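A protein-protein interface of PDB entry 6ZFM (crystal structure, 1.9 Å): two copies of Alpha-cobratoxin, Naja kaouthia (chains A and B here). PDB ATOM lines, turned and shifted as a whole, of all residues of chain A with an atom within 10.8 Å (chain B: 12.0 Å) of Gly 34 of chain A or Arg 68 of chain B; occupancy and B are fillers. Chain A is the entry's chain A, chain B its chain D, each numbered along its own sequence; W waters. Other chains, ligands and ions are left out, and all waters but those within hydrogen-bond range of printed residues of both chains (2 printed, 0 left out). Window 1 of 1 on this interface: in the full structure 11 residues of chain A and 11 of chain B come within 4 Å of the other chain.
The backbone carbonyl oxygen of Lys 69 of chain B lies close to the backbone carbonyl oxygen of Ser 31 of chain A, at 3.1 Å.
The side-chain amino group (NZ) of Lys 35 of chain A is in hydrogen-bond range of the backbone carbonyl oxygen (O) of Gly 51 of chain A (3.1 Å).
The backbone NH (N) of Lys 35 of chain A lies within hydrogen-bond range of the side-chain sulfur (SG) of Cys 30 of chain A, at 3.7 Å.
The side-chain hydroxyl (OG1) of Thr 67 of chain B is in hydrogen-bond range of the side-chain amino group (NZ) of Lys 69 of chain B.
The side-chain sulfur (SG) of Cys 26 of chain A is disulfide-bonded to the side-chain sulfur (SG) of Cys 30 of chain A (2.0 Å).
The guanidinium group (NE) of Arg 68 of chain B lies within salt-bridge range of the chain-end carboxylate (O) of Pro 71 of chain B.
Pro 71 of chain B touches Cys 26 of chain A.
O of Cys 30 of chain A touches O of Lys 69 of chain B, 3.9 Å away.
Cys 30 of chain A touches Arg 70 of chain B (O to CA, 3.6 Å).
CD of Pro 71 of chain B touches O of Cys 30 of chain A (3.6 Å).
Ile 32 of chain A touches Lys 69 of chain B (O to CG, 3.4 Å).
Arg 68 of chain B touches Arg 33 of chain A.
Arg 68 of chain B touches Gly 34 of chain A (O to CA, 3.2 Å).
Gly 34 of chain A touches Lys 69 of chain B.
Gly 34 of chain A touches Arg 70 of chain B.
Pro 71 of chain B touches Lys 35 of chain A.
Of chain B, only Pro 71 (3.6 Å) comes within 4 Å of Cys 26 of chain A.
Cys 30 of chain A touches just these residues of chain B: Lys 69 (3.9 Å), Arg 70 (3.6 Å) and Pro 71 (3.6 Å).
Of chain B, only Lys 69 comes within 4 Å of Ser 31 of chain A.
Of the printed residues of chain B, Ile 32 of chain A touches Lys 69 (3.4 Å).
Printed residues of chain B within 4 Å of Arg 33 of chain A: Arg 68.
Of chain B, only Pro 71 comes within 4 Å of Lys 35 of chain A.
Arg 36 of chain A touches none of the printed residues of chain B.
Lys 69 of chain B touches just these residues of chain A: Cys 30, Ser 31, Ile 32 and Gly 34.
Arg 70 of chain B touches just these residues of chain A: Cys 30 and Gly 34.
Pro 71 of chain B touches just these residues of chain A: Cys 26, Cys 30 and Lys 35.
The nearest residue of chain B that does not touch Gly 34 of chain A is Pro 71 of chain B (4.7 Å).
The nearest residue of chain A that does not touch Arg 68 of chain B is Lys 35 of chain A (4.7 Å).
Of the 18 printed residues of chain A, 7 touch a printed residue of chain B.
Printed residues of chain A that touch a printed residue of chain B: Cys 26, Cys 30, Ser 31, Ile 32, Arg 33, Gly 34 and Lys 35.
Printed residues of chain B that touch a printed residue of chain A: Arg 68, Lys 69, Arg 70 and Pro 71.
Hydrophobic or aromatic side chains of chain B that line the printed part of chain A: Pro 71.
Among the printed residues, no Asp or Glu carboxylate lies within 4 Å of a Lys or Arg side-chain nitrogen of the other chain.
Positions printed for both chains: 24, 35, 37 and 53.
Of the 11 pairs that touch across the chains among the printed residues, none has its exchanged pair printed and touching as well.
Water W1 lies within hydrogen-bond range of the side-chain hydroxyl (OG1) of Thr 67 of chain B (2.6 Å) and the backbone carbonyl oxygen (O) of Arg 33 of chain A (2.7 Å).
Water W2 lies within hydrogen-bond range of the backbone NH of Lys 35 of chain A (2.8 Å), the backbone carbonyl oxygen of Arg 70 of chain B (2.9 Å) and the backbone carbonyl oxygen of Arg 68 of chain B (3.4 Å).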
ATOM      1  N   LYS A  23     -15.129  -9.783 -19.853  1.00  0.00           N
ATOM      2  CA  LYS A  23     -15.793  -9.838 -18.560  1.00  0.00           C
ATOM      3  C   LYS A  23     -17.285  -9.688 -18.793  1.00  0.00           C
ATOM      4  O   LYS A  23     -17.724  -8.658 -19.310  1.00  0.00           O
ATOM      5  CB  LYS A  23     -15.282  -8.745 -17.621  1.00  0.00           C
ATOM      6  CG  LYS A  23     -16.126  -8.618 -16.358  1.00  0.00           C
ATOM      7  CD  LYS A  23     -15.372  -7.964 -15.212  1.00  0.00           C
ATOM      8  CE  LYS A  23     -15.488  -6.454 -15.241  1.00  0.00           C
ATOM      9  NZ  LYS A  23     -15.341  -5.884 -13.870  1.00  0.00           N
ATOM     10  N   THR A  24     -18.040 -10.724 -18.435  1.00  0.00           N
ATOM     11  CA  THR A  24     -19.489 -10.766 -18.572  1.00  0.00           C
ATOM     12  C   THR A  24     -20.073 -10.712 -17.169  1.00  0.00           C
ATOM     13  O   THR A  24     -19.767 -11.576 -16.336  1.00  0.00           O
ATOM     14  CB  THR A  24     -19.926 -12.036 -19.306  1.00  0.00           C
ATOM     15  OG1 THR A  24     -19.232 -12.143 -20.561  1.00  0.00           O
ATOM     16  CG2 THR A  24     -21.410 -12.035 -19.561  1.00  0.00           C
ATOM     17  N   TRP A  25     -20.902  -9.703 -16.903  1.00  0.00           N
ATOM     18  CA  TRP A  25     -21.306  -9.421 -15.532  1.00  0.00           C
ATOM     19  C   TRP A  25     -22.606  -8.620 -15.525  1.00  0.00           C
ATOM     20  O   TRP A  25     -23.043  -8.077 -16.545  1.00  0.00           O
ATOM     21  CB  TRP A  25     -20.203  -8.664 -14.776  1.00  0.00           C
ATOM     22  CG  TRP A  25     -19.899  -7.289 -15.338  1.00  0.00           C
ATOM     23  CD1 TRP A  25     -19.313  -7.002 -16.539  1.00  0.00           C
ATOM     24  CD2 TRP A  25     -20.164  -6.025 -14.710  1.00  0.00           C
ATOM     25  NE1 TRP A  25     -19.199  -5.638 -16.700  1.00  0.00           N
ATOM     26  CE2 TRP A  25     -19.712  -5.018 -15.590  1.00  0.00           C
ATOM     27  CE3 TRP A  25     -20.741  -5.649 -13.491  1.00  0.00           C
ATOM     28  CZ2 TRP A  25     -19.821  -3.657 -15.287  1.00  0.00           C
ATOM     29  CZ3 TRP A  25     -20.851  -4.296 -13.193  1.00  0.00           C
ATOM     30  CH2 TRP A  25     -20.393  -3.318 -14.088  1.00  0.00           C
ATOM     31  N   CYS A  26     -23.210  -8.549 -14.344  1.00  0.00           N
ATOM     32  CA  CYS A  26     -24.451  -7.812 -14.138  1.00  0.00           C
ATOM     33  C   CYS A  26     -24.121  -6.406 -13.648  1.00  0.00           C
ATOM     34  O   CYS A  26     -23.605  -6.238 -12.540  1.00  0.00           O
ATOM     35  CB  CYS A  26     -25.344  -8.530 -13.128  1.00  0.00           C
ATOM     36  SG  CYS A  26     -26.539  -9.715 -13.808  1.00  0.00           S
ATOM     37  N   ASP A  27     -24.410  -5.394 -14.466  1.00  0.00           N
ATOM     38  CA  ASP A  27     -24.345  -4.029 -13.972  1.00  0.00           C
ATOM     39  C   ASP A  27     -25.755  -3.590 -13.567  1.00  0.00           C
ATOM     40  O   ASP A  27     -26.648  -4.429 -13.395  1.00  0.00           O
ATOM     41  CB  ASP A  27     -23.671  -3.106 -15.002  1.00  0.00           C
ATOM     42  CG  ASP A  27     -24.538  -2.799 -16.207  1.00  0.00           C
ATOM     43  OD1 ASP A  27     -25.642  -3.373 -16.350  1.00  0.00           O
ATOM     44  OD2 ASP A  27     -24.092  -1.960 -17.024  1.00  0.00           O
ATOM     45  N   ALA A  28     -25.967  -2.277 -13.433  1.00  0.00           N
ATOM     46  CA  ALA A  28     -27.219  -1.756 -12.887  1.00  0.00           C
ATOM     47  C   ALA A  28     -28.436  -2.123 -13.729  1.00  0.00           C
ATOM     48  O   ALA A  28     -29.564  -2.086 -13.223  1.00  0.00           O
ATOM     49  CB  ALA A  28     -27.133  -0.233 -12.753  1.00  0.00           C
ATOM     50  N   PHE A  29     -28.235  -2.474 -14.996  1.00  0.00           N
ATOM     51  CA  PHE A  29     -29.326  -2.687 -15.934  1.00  0.00           C
ATOM     52  C   PHE A  29     -29.595  -4.161 -16.210  1.00  0.00           C
ATOM     53  O   PHE A  29     -30.323  -4.477 -17.161  1.00  0.00           O
ATOM     54  CB  PHE A  29     -29.026  -1.966 -17.245  1.00  0.00           C
ATOM     55  CG  PHE A  29     -28.704  -0.511 -17.077  1.00  0.00           C
ATOM     56  CD1 PHE A  29     -29.721   0.435 -16.995  1.00  0.00           C
ATOM     57  CD2 PHE A  29     -27.391  -0.081 -17.011  1.00  0.00           C
ATOM     58  CE1 PHE A  29     -29.426   1.780 -16.850  1.00  0.00           C
ATOM     59  CE2 PHE A  29     -27.089   1.265 -16.864  1.00  0.00           C
ATOM     60  CZ  PHE A  29     -28.107   2.194 -16.783  1.00  0.00           C
ATOM     61  N   CYS A  30     -29.038  -5.064 -15.392  1.00  0.00           N
ATOM     62  CA  CYS A  30     -29.101  -6.492 -15.696  1.00  0.00           C
ATOM     63  C   CYS A  30     -30.543  -6.975 -15.813  1.00  0.00           C
ATOM     64  O   CYS A  30     -30.861  -7.808 -16.672  1.00  0.00           O
ATOM     65  CB  CYS A  30     -28.346  -7.294 -14.632  1.00  0.00           C
ATOM     66  SG  CYS A  30     -27.510  -8.738 -15.326  1.00  0.00           S
ATOM     67  N   SER A  31     -31.432  -6.457 -14.964  1.00  0.00           N
ATOM     68  CA  SER A  31     -32.828  -6.876 -15.000  1.00  0.00           C
ATOM     69  C   SER A  31     -33.538  -6.429 -16.272  1.00  0.00           C
ATOM     70  O   SER A  31     -34.563  -7.017 -16.631  1.00  0.00           O
ATOM     71  CB  SER A  31     -33.562  -6.336 -13.774  1.00  0.00           C
ATOM     72  OG  SER A  31     -33.541  -4.920 -13.779  1.00  0.00           O
ATOM     73  N   ILE A  32     -33.023  -5.409 -16.954  1.00  0.00           N
ATOM     74  CA  ILE A  32     -33.615  -4.906 -18.186  1.00  0.00           C
ATOM     75  C   ILE A  32     -32.861  -5.403 -19.414  1.00  0.00           C
ATOM     76  O   ILE A  32     -33.471  -5.794 -20.411  1.00  0.00           O
ATOM     77  CB  ILE A  32     -33.648  -3.363 -18.165  1.00  0.00           C
ATOM     78  CG1 ILE A  32     -34.310  -2.843 -16.890  1.00  0.00           C
ATOM     79  CG2 ILE A  32     -34.360  -2.834 -19.393  1.00  0.00           C
ATOM     80  CD1 ILE A  32     -34.210  -1.341 -16.743  1.00  0.00           C
ATOM     81  N   ARG A  33     -31.530  -5.383 -19.355  1.00  0.00           N
ATOM     82  CA  ARG A  33     -30.702  -5.624 -20.525  1.00  0.00           C
ATOM     83  C   ARG A  33     -29.992  -6.967 -20.513  1.00  0.00           C
ATOM     84  O   ARG A  33     -29.504  -7.393 -21.565  1.00  0.00           O
ATOM     85  CB  ARG A  33     -29.641  -4.522 -20.659  1.00  0.00           C
ATOM     86  CG  ARG A  33     -30.201  -3.096 -20.643  1.00  0.00           C
ATOM     87  CD  ARG A  33     -29.080  -2.072 -20.841  1.00  0.00           C
ATOM     88  NE  ARG A  33     -29.514  -0.693 -20.600  1.00  0.00           N
ATOM     89  CZ  ARG A  33     -28.685   0.350 -20.558  1.00  0.00           C
ATOM     90  NH1 ARG A  33     -27.377   0.173 -20.733  1.00  0.00           N
ATOM     91  NH2 ARG A  33     -29.160   1.569 -20.333  1.00  0.00           N
ATOM     92  N   GLY A  34     -29.923  -7.638 -19.371  1.00  0.00           N
ATOM     93  CA  GLY A  34     -29.060  -8.792 -19.240  1.00  0.00           C
ATOM     94  C   GLY A  34     -27.639  -8.364 -18.916  1.00  0.00           C
ATOM     95  O   GLY A  34     -27.349  -7.189 -18.670  1.00  0.00           O
ATOM     96  N   LYS A  35     -26.741  -9.345 -18.909  1.00  0.00           N
ATOM     97  CA  LYS A  35     -25.369  -9.086 -18.499  1.00  0.00           C
ATOM     98  C   LYS A  35     -24.631  -8.222 -19.520  1.00  0.00           C
ATOM     99  O   LYS A  35     -24.820  -8.355 -20.734  1.00  0.00           O
ATOM    100  CB  LYS A  35     -24.620 -10.406 -18.268  1.00  0.00           C
ATOM    101  CG  LYS A  35     -25.149 -11.184 -17.060  1.00  0.00           C
ATOM    102  CD  LYS A  35     -24.320 -12.423 -16.745  1.00  0.00           C
ATOM    103  CE  LYS A  35     -24.778 -13.060 -15.433  1.00  0.00           C
ATOM    104  NZ  LYS A  35     -23.858 -14.167 -15.023  1.00  0.00           N
ATOM    105  N   ARG A  36     -23.819  -7.302 -19.005  1.00  0.00           N
ATOM    106  CA  ARG A  36     -22.876  -6.544 -19.811  1.00  0.00           C
ATOM    107  C   ARG A  36     -21.702  -7.439 -20.203  1.00  0.00           C
ATOM    108  O   ARG A  36     -21.322  -8.348 -19.462  1.00  0.00           O
ATOM    109  CB  ARG A  36     -22.378  -5.334 -19.018  1.00  0.00           C
ATOM    110  CG  ARG A  36     -21.682  -4.265 -19.837  1.00  0.00           C
ATOM    111  CD  ARG A  36     -21.303  -3.077 -18.962  1.00  0.00           C
ATOM    112  NE  ARG A  36     -20.389  -2.168 -19.646  1.00  0.00           N
ATOM    113  CZ  ARG A  36     -20.714  -0.946 -20.050  1.00  0.00           C
ATOM    114  NH1 ARG A  36     -21.934  -0.470 -19.819  1.00  0.00           N
ATOM    115  NH2 ARG A  36     -19.817  -0.192 -20.669  1.00  0.00           N
ATOM    116  N   VAL A  37     -21.138  -7.193 -21.386  1.00  0.00           N
ATOM    117  CA  VAL A  37     -19.976  -7.941 -21.886  1.00  0.00           C
ATOM    118  C   VAL A  37     -18.906  -6.917 -22.249  1.00  0.00           C
ATOM    119  O   VAL A  37     -18.997  -6.259 -23.291  1.00  0.00           O
ATOM    120  CB  VAL A  37     -20.320  -8.826 -23.092  1.00  0.00           C
ATOM    121  CG1 VAL A  37     -19.100  -9.641 -23.534  1.00  0.00           C
ATOM    122  CG2 VAL A  37     -21.484  -9.747 -22.769  1.00  0.00           C
ATOM    123  N   ASP A  38     -17.887  -6.782 -21.403  1.00  0.00           N
ATOM    124  CA  ASP A  38     -16.806  -5.829 -21.626  1.00  0.00           C
ATOM    125  C   ASP A  38     -15.567  -6.537 -22.162  1.00  0.00           C
ATOM    126  O   ASP A  38     -15.253  -7.656 -21.750  1.00  0.00           O
ATOM    127  CB  ASP A  38     -16.447  -5.092 -20.336  1.00  0.00           C
ATOM    128  CG  ASP A  38     -17.545  -4.154 -19.871  1.00  0.00           C
ATOM    129  OD1 ASP A  38     -18.056  -3.357 -20.695  1.00  0.00           O
ATOM    130  OD2 ASP A  38     -17.899  -4.219 -18.676  1.00  0.00           O
ATOM    131  N   GLY A  51     -21.264 -14.829 -10.324  1.00  0.00           N
ATOM    132  CA  GLY A  51     -21.950 -14.083 -11.364  1.00  0.00           C
ATOM    133  C   GLY A  51     -21.104 -13.490 -12.470  1.00  0.00           C
ATOM    134  O   GLY A  51     -21.643 -12.757 -13.311  1.00  0.00           O
ATOM    135  N   ASP A  53     -18.337 -14.196 -15.574  1.00  0.00           N
ATOM    136  CA  ASP A  53     -17.584 -15.081 -16.459  1.00  0.00           C
ATOM    137  C   ASP A  53     -16.446 -14.292 -17.091  1.00  0.00           C
ATOM    138  O   ASP A  53     -16.672 -13.214 -17.656  1.00  0.00           O
ATOM    139  CB  ASP A  53     -18.469 -15.677 -17.557  1.00  0.00           C
ATOM    140  CG  ASP A  53     -19.738 -16.301 -17.013  1.00  0.00           C
ATOM    141  OD1 ASP A  53     -19.643 -17.141 -16.093  1.00  0.00           O
ATOM    142  OD2 ASP A  53     -20.834 -15.943 -17.505  1.00  0.00           O
ATOM    143  N   THR B  22     -36.728 -14.132 -35.666  1.00  0.00           N
ATOM    144  CA  THR B  22     -35.378 -14.568 -35.343  1.00  0.00           C
ATOM    145  C   THR B  22     -35.404 -16.081 -35.206  1.00  0.00           C
ATOM    146  O   THR B  22     -36.437 -16.670 -34.861  1.00  0.00           O
ATOM    147  CB  THR B  22     -34.844 -13.941 -34.040  1.00  0.00           C
ATOM    148  OG1 THR B  22     -35.398 -14.629 -32.904  1.00  0.00           O
ATOM    149  CG2 THR B  22     -35.191 -12.447 -33.967  1.00  0.00           C
ATOM    150  N   THR B  24     -32.671 -19.175 -33.834  1.00  0.00           N
ATOM    151  CA  THR B  24     -31.398 -19.632 -33.291  1.00  0.00           C
ATOM    152  C   THR B  24     -31.395 -21.149 -33.356  1.00  0.00           C
ATOM    153  O   THR B  24     -32.287 -21.795 -32.792  1.00  0.00           O
ATOM    154  CB  THR B  24     -31.200 -19.157 -31.853  1.00  0.00           C
ATOM    155  OG1 THR B  24     -31.383 -17.737 -31.783  1.00  0.00           O
ATOM    156  CG2 THR B  24     -29.807 -19.503 -31.363  1.00  0.00           C
ATOM    157  N   LYS B  35     -24.628 -22.110 -32.028  1.00  0.00           N
ATOM    158  CA  LYS B  35     -25.847 -21.960 -32.810  1.00  0.00           C
ATOM    159  C   LYS B  35     -25.769 -20.740 -33.729  1.00  0.00           C
ATOM    160  O   LYS B  35     -25.217 -19.698 -33.370  1.00  0.00           O
ATOM    161  CB  LYS B  35     -27.070 -21.856 -31.888  1.00  0.00           C
ATOM    162  CG  LYS B  35     -27.356 -23.162 -31.140  1.00  0.00           C
ATOM    163  CD  LYS B  35     -28.639 -23.103 -30.333  1.00  0.00           C
ATOM    164  CE  LYS B  35     -28.974 -24.474 -29.755  1.00  0.00           C
ATOM    165  NZ  LYS B  35     -30.328 -24.478 -29.114  1.00  0.00           N
ATOM    166  N   VAL B  37     -27.633 -17.655 -35.644  1.00  0.00           N
ATOM    167  CA  VAL B  37     -28.717 -16.732 -35.290  1.00  0.00           C
ATOM    168  C   VAL B  37     -29.092 -15.972 -36.556  1.00  0.00           C
ATOM    169  O   VAL B  37     -28.367 -15.064 -36.980  1.00  0.00           O
ATOM    170  CB  VAL B  37     -28.327 -15.764 -34.165  1.00  0.00           C
ATOM    171  CG1 VAL B  37     -29.520 -14.876 -33.792  1.00  0.00           C
ATOM    172  CG2 VAL B  37     -27.839 -16.524 -32.948  1.00  0.00           C
ATOM    173  N   ASP B  53     -34.818 -21.947 -31.126  1.00  0.00           N
ATOM    174  CA  ASP B  53     -35.465 -20.847 -30.420  1.00  0.00           C
ATOM    175  C   ASP B  53     -35.936 -19.829 -31.447  1.00  0.00           C
ATOM    176  O   ASP B  53     -35.159 -19.423 -32.321  1.00  0.00           O
ATOM    177  CB  ASP B  53     -34.516 -20.174 -29.426  1.00  0.00           C
ATOM    178  CG  ASP B  53     -33.818 -21.165 -28.516  1.00  0.00           C
ATOM    179  OD1 ASP B  53     -34.514 -21.988 -27.883  1.00  0.00           O
ATOM    180  OD2 ASP B  53     -32.569 -21.123 -28.439  1.00  0.00           O
ATOM    181  N   GLN B  55     -38.396 -16.259 -32.368  1.00  0.00           N
ATOM    182  CA  GLN B  55     -39.234 -15.096 -32.125  1.00  0.00           C
ATOM    183  C   GLN B  55     -39.924 -14.717 -33.428  1.00  0.00           C
ATOM    184  O   GLN B  55     -39.327 -14.814 -34.503  1.00  0.00           O
ATOM    185  CB  GLN B  55     -38.423 -13.915 -31.590  1.00  0.00           C
ATOM    186  CG  GLN B  55     -37.744 -14.177 -30.256  1.00  0.00           C
ATOM    187  CD  GLN B  55     -36.685 -13.136 -29.921  1.00  0.00           C
ATOM    188  OE1 GLN B  55     -36.001 -12.620 -30.803  1.00  0.00           O
ATOM    189  NE2 GLN B  55     -36.551 -12.822 -28.639  1.00  0.00           N
ATOM    190  N   PRO B  64     -34.724  -7.531 -33.837  1.00  0.00           N
ATOM    191  CA  PRO B  64     -33.270  -7.352 -33.705  1.00  0.00           C
ATOM    192  C   PRO B  64     -32.654  -8.627 -33.149  1.00  0.00           C
ATOM    193  O   PRO B  64     -33.389  -9.562 -32.816  1.00  0.00           O
ATOM    194  CB  PRO B  64     -33.141  -6.174 -32.736  1.00  0.00           C
ATOM    195  CG  PRO B  64     -34.364  -6.303 -31.844  1.00  0.00           C
ATOM    196  CD  PRO B  64     -35.462  -6.873 -32.735  1.00  0.00           C
ATOM    197  N   PHE B  65     -31.331  -8.697 -33.038  1.00  0.00           N
ATOM    198  CA  PHE B  65     -30.711  -9.896 -32.485  1.00  0.00           C
ATOM    199  C   PHE B  65     -31.266 -10.166 -31.093  1.00  0.00           C
ATOM    200  O   PHE B  65     -31.392  -9.229 -30.292  1.00  0.00           O
ATOM    201  CB  PHE B  65     -29.190  -9.759 -32.419  1.00  0.00           C
ATOM    202  CG  PHE B  65     -28.513  -9.955 -33.741  1.00  0.00           C
ATOM    203  CD1 PHE B  65     -28.471 -11.217 -34.328  1.00  0.00           C
ATOM    204  CD2 PHE B  65     -27.919  -8.894 -34.395  1.00  0.00           C
ATOM    205  CE1 PHE B  65     -27.839 -11.411 -35.561  1.00  0.00           C
ATOM    206  CE2 PHE B  65     -27.282  -9.080 -35.621  1.00  0.00           C
ATOM    207  CZ  PHE B  65     -27.250 -10.347 -36.202  1.00  0.00           C
ATOM    208  N   PRO B  66     -31.623 -11.409 -30.776  1.00  0.00           N
ATOM    209  CA  PRO B  66     -32.145 -11.717 -29.439  1.00  0.00           C
ATOM    210  C   PRO B  66     -31.102 -11.512 -28.354  1.00  0.00           C
ATOM    211  O   PRO B  66     -29.901 -11.665 -28.576  1.00  0.00           O
ATOM    212  CB  PRO B  66     -32.535 -13.200 -29.537  1.00  0.00           C
ATOM    213  CG  PRO B  66     -32.654 -13.482 -30.995  1.00  0.00           C
ATOM    214  CD  PRO B  66     -31.654 -12.577 -31.669  1.00  0.00           C
ATOM    215  N   THR B  67     -31.585 -11.174 -27.162  1.00  0.00           N
ATOM    216  CA  THR B  67     -30.756 -11.131 -25.967  1.00  0.00           C
ATOM    217  C   THR B  67     -31.534 -11.767 -24.831  1.00  0.00           C
ATOM    218  O   THR B  67     -32.764 -11.855 -24.868  1.00  0.00           O
ATOM    219  CB  THR B  67     -30.354  -9.705 -25.548  1.00  0.00           C
ATOM    220  OG1 THR B  67     -31.531  -8.902 -25.347  1.00  0.00           O
ATOM    221  CG2 THR B  67     -29.439  -9.059 -26.596  1.00  0.00           C
ATOM    222  N   ARG B  68     -30.801 -12.206 -23.818  1.00  0.00           N
ATOM    223  CA  ARG B  68     -31.392 -12.631 -22.557  1.00  0.00           C
ATOM    224  C   ARG B  68     -31.564 -11.385 -21.692  1.00  0.00           C
ATOM    225  O   ARG B  68     -30.578 -10.817 -21.211  1.00  0.00           O
ATOM    226  CB  ARG B  68     -30.508 -13.679 -21.884  1.00  0.00           C
ATOM    227  CG  ARG B  68     -31.070 -14.272 -20.602  1.00  0.00           C
ATOM    228  CD  ARG B  68     -30.118 -15.316 -20.034  1.00  0.00           C
ATOM    229  NE  ARG B  68     -30.560 -15.830 -18.736  1.00  0.00           N
ATOM    230  CZ  ARG B  68     -31.428 -16.825 -18.576  1.00  0.00           C
ATOM    231  NH1 ARG B  68     -31.765 -17.224 -17.357  1.00  0.00           N
ATOM    232  NH2 ARG B  68     -31.963 -17.420 -19.634  1.00  0.00           N
ATOM    233  N   LYS B  69     -32.815 -10.941 -21.520  1.00  0.00           N
ATOM    234  CA  LYS B  69     -33.112  -9.713 -20.776  1.00  0.00           C
ATOM    235  C   LYS B  69     -33.148  -9.924 -19.272  1.00  0.00           C
ATOM    236  O   LYS B  69     -33.970  -9.323 -18.574  1.00  0.00           O
ATOM    237  CB  LYS B  69     -34.433  -9.117 -21.259  1.00  0.00           C
ATOM    238  CG  LYS B  69     -34.329  -8.294 -22.522  1.00  0.00           C
ATOM    239  CD  LYS B  69     -34.458  -9.165 -23.746  1.00  0.00           C
ATOM    240  CE  LYS B  69     -34.571  -8.322 -24.995  1.00  0.00           C
ATOM    241  NZ  LYS B  69     -34.323  -9.160 -26.192  1.00  0.00           N
ATOM    242  N   ARG B  70     -32.265 -10.767 -18.748  1.00  0.00           N
ATOM    243  CA  ARG B  70     -32.209 -11.052 -17.323  1.00  0.00           C
ATOM    244  C   ARG B  70     -30.856 -11.677 -17.023  1.00  0.00           C
ATOM    245  O   ARG B  70     -30.198 -12.199 -17.932  1.00  0.00           O
ATOM    246  CB  ARG B  70     -33.354 -11.987 -16.900  1.00  0.00           C
ATOM    247  CG  ARG B  70     -33.376 -13.320 -17.631  1.00  0.00           C
ATOM    248  CD  ARG B  70     -34.560 -14.166 -17.190  1.00  0.00           C
ATOM    249  NE  ARG B  70     -34.532 -15.501 -17.780  1.00  0.00           N
ATOM    250  CZ  ARG B  70     -34.985 -15.790 -18.996  1.00  0.00           C
ATOM    251  NH1 ARG B  70     -34.922 -17.034 -19.452  1.00  0.00           N
ATOM    252  NH2 ARG B  70     -35.495 -14.834 -19.762  1.00  0.00           N
ATOM    253  N   PRO B  71     -30.399 -11.622 -15.756  1.00  0.00           N
ATOM    254  CA  PRO B  71     -29.157 -12.281 -15.334  1.00  0.00           C
ATOM    255  C   PRO B  71     -29.056 -13.744 -15.775  1.00  0.00           C
ATOM    256  O   PRO B  71     -30.060 -14.408 -16.038  1.00  0.00           O
ATOM    257  CB  PRO B  71     -29.215 -12.178 -13.808  1.00  0.00           C
ATOM    258  CG  PRO B  71     -29.959 -10.910 -13.562  1.00  0.00           C
ATOM    259  CD  PRO B  71     -30.977 -10.799 -14.675  1.00  0.00           C
ATOM    260  OXT PRO B  71     -27.961 -14.296 -15.881  1.00  0.00           O
HETATM  261  O   HOH W   1     -30.783  -6.897 -23.925  1.00  0.00           O
HETATM  262  O   HOH W   2     -27.777 -11.834 -19.541  1.00  0.00           O
